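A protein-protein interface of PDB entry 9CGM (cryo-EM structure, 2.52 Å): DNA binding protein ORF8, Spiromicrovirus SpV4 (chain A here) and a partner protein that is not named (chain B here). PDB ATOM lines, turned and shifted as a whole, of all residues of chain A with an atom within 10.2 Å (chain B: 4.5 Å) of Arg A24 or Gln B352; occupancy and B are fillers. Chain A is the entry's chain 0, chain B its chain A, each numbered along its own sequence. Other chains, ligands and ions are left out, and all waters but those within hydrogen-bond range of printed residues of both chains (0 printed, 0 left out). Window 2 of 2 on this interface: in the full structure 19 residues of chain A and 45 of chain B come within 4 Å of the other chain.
Of the printed residues of chain B, Ile A22 touches Ile B79 (3.6 Å) and Ser B353 (3.9 Å).
Lys A23 touches none of the printed residues of chain B.
Arg A24 touches just these residues of chain B: His B350, Ser B351 and Gln B352.
Printed residues of chain B within 4 Å of Ala A25: His B350 and Ser B351.
Asn A26 touches none of the printed residues of chain B.
Of the printed residues of chain B, Ile A27 touches His B350 (3.3 Å).
Of the printed residues of chain A, Ile B79 touches Ile A22.
No residue of chain A comes within 4 Å of Val B80.
Printed residues of chain A within 4 Å of His B350: Arg A24, Ala A25 and Ile A27.
Of chain A, only Arg A24 (3.2 Å) and Ala A25 (2.9 Å) come within 4 Å of Ser B351.
Gln B352 touches just one residue of chain A: Arg A24 (3.7 Å).
Ser B353 touches just one residue of chain A: Ile A22.
The nearest printed residue of chain A that does not touch Ile B79 is Lys A23 (6.9 Å).
Ile A22 touches Ile B79.
OG of Ser B353 touches O of Ile A22, 3.9 Å away.
CE1 of His B350 touches CB of Arg A24, 3.8 Å away.
Arg A24 touches Ser B351.
NH2 of Arg A24 touches NE2 of Gln B352, at 3.7 Å.
His B350 touches Ile A27 (O to CD1, 3.3 Å).
A ring nitrogen (ND1) of His B350 is in hydrogen-bond range of the backbone carbonyl oxygen (O) of Ala A25.
N of Ser B351 lies within hydrogen-bond range of O of Ala A25 (2.9 Å).
Printed residues of chain B that touch a printed residue of chain A: Ile B79, His B350, Ser B351, Gln B352 and Ser B353.
Of the 7 printed residues of chain A, 4 touch a printed residue of chain B.
Printed residues of chain A that touch a printed residue of chain B: Ile A22, Arg A24, Ala A25 and Ile A27.
Hydrophobic or aromatic side chains of chain A that line the printed part of chain B: Ile A22 and Ile A27.
Among the printed residues, no Asp or Glu carboxylate lies within 4 Å of a Lys or Arg side-chain nitrogen of the other chain.
The backbone NH of Val B80 lies within hydrogen-bond range of the backbone carbonyl oxygen of Gln B352, at 2.8 Å.
A ring nitrogen (NE2) of His B350 sits at hydrogen-bond distance from the side-chain amide oxygen (OE1) of Gln B352.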
ATOM      1  N   SER A  21     -30.067 -19.593  11.437  1.00  0.00           N
ATOM      2  CA  SER A  21     -28.921 -20.048  12.205  1.00  0.00           C
ATOM      3  C   SER A  21     -28.060 -20.946  11.333  1.00  0.00           C
ATOM      4  O   SER A  21     -28.564 -21.639  10.446  1.00  0.00           O
ATOM      5  CB  SER A  21     -29.351 -20.793  13.467  1.00  0.00           C
ATOM      6  OG  SER A  21     -30.056 -21.974  13.152  1.00  0.00           O
ATOM      7  N   ILE A  22     -26.757 -20.919  11.579  1.00  0.00           N
ATOM      8  CA  ILE A  22     -25.791 -21.693  10.814  1.00  0.00           C
ATOM      9  C   ILE A  22     -25.022 -22.573  11.779  1.00  0.00           C
ATOM     10  O   ILE A  22     -24.553 -22.101  12.819  1.00  0.00           O
ATOM     11  CB  ILE A  22     -24.852 -20.779  10.008  1.00  0.00           C
ATOM     12  CG1 ILE A  22     -25.652 -20.091   8.906  1.00  0.00           C
ATOM     13  CG2 ILE A  22     -23.697 -21.559   9.426  1.00  0.00           C
ATOM     14  CD1 ILE A  22     -24.902 -19.062   8.159  1.00  0.00           C
ATOM     15  N   LYS A  23     -24.907 -23.849  11.446  1.00  0.00           N
ATOM     16  CA  LYS A  23     -24.311 -24.825  12.342  1.00  0.00           C
ATOM     17  C   LYS A  23     -22.864 -25.075  11.949  1.00  0.00           C
ATOM     18  O   LYS A  23     -22.535 -25.137  10.763  1.00  0.00           O
ATOM     19  CB  LYS A  23     -25.109 -26.128  12.321  1.00  0.00           C
ATOM     20  CG  LYS A  23     -24.664 -27.141  13.351  1.00  0.00           C
ATOM     21  CD  LYS A  23     -25.539 -28.379  13.316  1.00  0.00           C
ATOM     22  CE  LYS A  23     -25.092 -29.399  14.350  1.00  0.00           C
ATOM     23  NZ  LYS A  23     -25.939 -30.621  14.326  1.00  0.00           N
ATOM     24  N   ARG A  24     -22.001 -25.199  12.950  1.00  0.00           N
ATOM     25  CA  ARG A  24     -20.602 -25.488  12.688  1.00  0.00           C
ATOM     26  C   ARG A  24     -20.463 -26.917  12.174  1.00  0.00           C
ATOM     27  O   ARG A  24     -21.255 -27.799  12.508  1.00  0.00           O
ATOM     28  CB  ARG A  24     -19.766 -25.286  13.951  1.00  0.00           C
ATOM     29  CG  ARG A  24     -19.911 -26.397  14.943  1.00  0.00           C
ATOM     30  CD  ARG A  24     -19.017 -26.258  16.156  1.00  0.00           C
ATOM     31  NE  ARG A  24     -19.448 -25.166  17.019  1.00  0.00           N
ATOM     32  CZ  ARG A  24     -18.764 -24.727  18.067  1.00  0.00           C
ATOM     33  NH1 ARG A  24     -17.622 -25.306  18.398  1.00  0.00           N
ATOM     34  NH2 ARG A  24     -19.235 -23.728  18.798  1.00  0.00           N
ATOM     35  N   ALA A  25     -19.458 -27.141  11.333  1.00  0.00           N
ATOM     36  CA  ALA A  25     -19.333 -28.432  10.682  1.00  0.00           C
ATOM     37  C   ALA A  25     -17.877 -28.731  10.369  1.00  0.00           C
ATOM     38  O   ALA A  25     -17.084 -27.829  10.104  1.00  0.00           O
ATOM     39  CB  ALA A  25     -20.161 -28.480   9.398  1.00  0.00           C
ATOM     40  N   ASN A  26     -17.538 -30.015  10.405  1.00  0.00           N
ATOM     41  CA  ASN A  26     -16.291 -30.468   9.813  1.00  0.00           C
ATOM     42  C   ASN A  26     -16.408 -30.459   8.301  1.00  0.00           C
ATOM     43  O   ASN A  26     -17.434 -30.845   7.741  1.00  0.00           O
ATOM     44  CB  ASN A  26     -15.935 -31.867  10.297  1.00  0.00           C
ATOM     45  CG  ASN A  26     -15.379 -31.870  11.693  1.00  0.00           C
ATOM     46  OD1 ASN A  26     -14.798 -30.883  12.147  1.00  0.00           O
ATOM     47  ND2 ASN A  26     -15.562 -32.976  12.397  1.00  0.00           N
ATOM     48  N   ILE A  27     -15.356 -30.011   7.641  1.00  0.00           N
ATOM     49  CA  ILE A  27     -15.315 -29.981   6.189  1.00  0.00           C
ATOM     50  C   ILE A  27     -14.815 -31.327   5.694  1.00  0.00           C
ATOM     51  O   ILE A  27     -13.860 -31.885   6.241  1.00  0.00           O
ATOM     52  CB  ILE A  27     -14.425 -28.835   5.690  1.00  0.00           C
ATOM     53  CG1 ILE A  27     -15.020 -27.495   6.114  1.00  0.00           C
ATOM     54  CG2 ILE A  27     -14.271 -28.902   4.186  1.00  0.00           C
ATOM     55  CD1 ILE A  27     -14.125 -26.329   5.872  1.00  0.00           C
ATOM     56  N   LEU B  78     -21.704 -14.109   8.432  1.00  0.00           N
ATOM     57  CA  LEU B  78     -20.364 -14.331   7.898  1.00  0.00           C
ATOM     58  C   LEU B  78     -19.844 -15.672   8.391  1.00  0.00           C
ATOM     59  O   LEU B  78     -19.986 -15.997   9.572  1.00  0.00           O
ATOM     60  CB  LEU B  78     -19.401 -13.222   8.318  1.00  0.00           C
ATOM     61  CG  LEU B  78     -19.593 -11.822   7.755  1.00  0.00           C
ATOM     62  CD1 LEU B  78     -18.606 -10.883   8.384  1.00  0.00           C
ATOM     63  CD2 LEU B  78     -19.421 -11.830   6.259  1.00  0.00           C
ATOM     64  N   ILE B  79     -19.229 -16.438   7.497  1.00  0.00           N
ATOM     65  CA  ILE B  79     -18.826 -17.812   7.775  1.00  0.00           C
ATOM     66  C   ILE B  79     -17.334 -17.945   7.506  1.00  0.00           C
ATOM     67  O   ILE B  79     -16.843 -17.471   6.479  1.00  0.00           O
ATOM     68  CB  ILE B  79     -19.626 -18.805   6.916  1.00  0.00           C
ATOM     69  CG1 ILE B  79     -21.119 -18.622   7.155  1.00  0.00           C
ATOM     70  CG2 ILE B  79     -19.240 -20.223   7.251  1.00  0.00           C
ATOM     71  CD1 ILE B  79     -21.974 -19.250   6.105  1.00  0.00           C
ATOM     72  N   VAL B  80     -16.620 -18.586   8.420  1.00  0.00           N
ATOM     73  CA  VAL B  80     -15.188 -18.829   8.286  1.00  0.00           C
ATOM     74  C   VAL B  80     -14.975 -20.283   7.893  1.00  0.00           C
ATOM     75  O   VAL B  80     -15.591 -21.181   8.471  1.00  0.00           O
ATOM     76  CB  VAL B  80     -14.438 -18.507   9.592  1.00  0.00           C
ATOM     77  CG1 VAL B  80     -12.995 -18.903   9.480  1.00  0.00           C
ATOM     78  CG2 VAL B  80     -14.542 -17.048   9.926  1.00  0.00           C
ATOM     79  N   HIS B 350     -12.664 -27.002   9.045  1.00  0.00           N
ATOM     80  CA  HIS B 350     -13.772 -26.658   9.917  1.00  0.00           C
ATOM     81  C   HIS B 350     -14.467 -25.427   9.364  1.00  0.00           C
ATOM     82  O   HIS B 350     -13.854 -24.604   8.688  1.00  0.00           O
ATOM     83  CB  HIS B 350     -13.273 -26.412  11.339  1.00  0.00           C
ATOM     84  CG  HIS B 350     -14.343 -26.039  12.310  1.00  0.00           C
ATOM     85  ND1 HIS B 350     -15.341 -26.906  12.691  1.00  0.00           N
ATOM     86  CD2 HIS B 350     -14.580 -24.881  12.968  1.00  0.00           C
ATOM     87  CE1 HIS B 350     -16.140 -26.302  13.551  1.00  0.00           C
ATOM     88  NE2 HIS B 350     -15.700 -25.071  13.735  1.00  0.00           N
ATOM     89  N   SER B 351     -15.750 -25.305   9.665  1.00  0.00           N
ATOM     90  CA  SER B 351     -16.566 -24.206   9.182  1.00  0.00           C
ATOM     91  C   SER B 351     -17.439 -23.689  10.314  1.00  0.00           C
ATOM     92  O   SER B 351     -18.095 -24.472  11.000  1.00  0.00           O
ATOM     93  CB  SER B 351     -17.432 -24.661   8.015  1.00  0.00           C
ATOM     94  OG  SER B 351     -18.204 -23.595   7.512  1.00  0.00           O
ATOM     95  N   GLN B 352     -17.427 -22.375  10.528  1.00  0.00           N
ATOM     96  CA  GLN B 352     -18.223 -21.787  11.598  1.00  0.00           C
ATOM     97  C   GLN B 352     -18.588 -20.347  11.261  1.00  0.00           C
ATOM     98  O   GLN B 352     -17.775 -19.613  10.699  1.00  0.00           O
ATOM     99  CB  GLN B 352     -17.456 -21.862  12.920  1.00  0.00           C
ATOM    100  CG  GLN B 352     -18.194 -21.362  14.116  1.00  0.00           C
ATOM    101  CD  GLN B 352     -17.496 -21.710  15.400  1.00  0.00           C
ATOM    102  OE1 GLN B 352     -16.565 -22.503  15.415  1.00  0.00           O
ATOM    103  NE2 GLN B 352     -17.924 -21.099  16.486  1.00  0.00           N
ATOM    104  N   SER B 353     -19.810 -19.954  11.614  1.00  0.00           N
ATOM    105  CA  SER B 353     -20.255 -18.572  11.512  1.00  0.00           C
ATOM    106  C   SER B 353     -19.707 -17.730  12.665  1.00  0.00           C
ATOM    107  O   SER B 353     -19.259 -18.240  13.692  1.00  0.00           O
ATOM    108  CB  SER B 353     -21.777 -18.489  11.471  1.00  0.00           C
ATOM    109  OG  SER B 353     -22.358 -18.904  12.687  1.00  0.00           O
ATOM    110  N   LEU B 354     -19.748 -16.417  12.481  1.00  0.00           N
ATOM    111  CA  LEU B 354     -19.228 -15.455  13.441  1.00  0.00           C
ATOM    112  C   LEU B 354     -20.348 -14.864  14.287  1.00  0.00           C
ATOM    113  O   LEU B 354     -21.478 -14.701  13.828  1.00  0.00           O
ATOM    114  CB  LEU B 354     -18.486 -14.331  12.726  1.00  0.00           C
ATOM    115  CG  LEU B 354     -17.277 -14.764  11.909  1.00  0.00           C
ATOM    116  CD1 LEU B 354     -16.679 -13.575  11.209  1.00  0.00           C
ATOM    117  CD2 LEU B 354     -16.251 -15.455  12.775  1.00  0.00           C
ATOM    118  N   ILE B 383     -12.820 -19.302  17.796  1.00  0.00           N
ATOM    119  CA  ILE B 383     -13.044 -20.586  17.147  1.00  0.00           C
ATOM    120  C   ILE B 383     -11.910 -21.526  17.522  1.00  0.00           C
ATOM    121  O   ILE B 383     -10.739 -21.141  17.484  1.00  0.00           O
ATOM    122  CB  ILE B 383     -13.145 -20.443  15.621  1.00  0.00           C
ATOM    123  CG1 ILE B 383     -14.317 -19.546  15.255  1.00  0.00           C
ATOM    124  CG2 ILE B 383     -13.337 -21.793  14.983  1.00  0.00           C
ATOM    125  CD1 ILE B 383     -14.374 -19.220  13.799  1.00  0.00           C
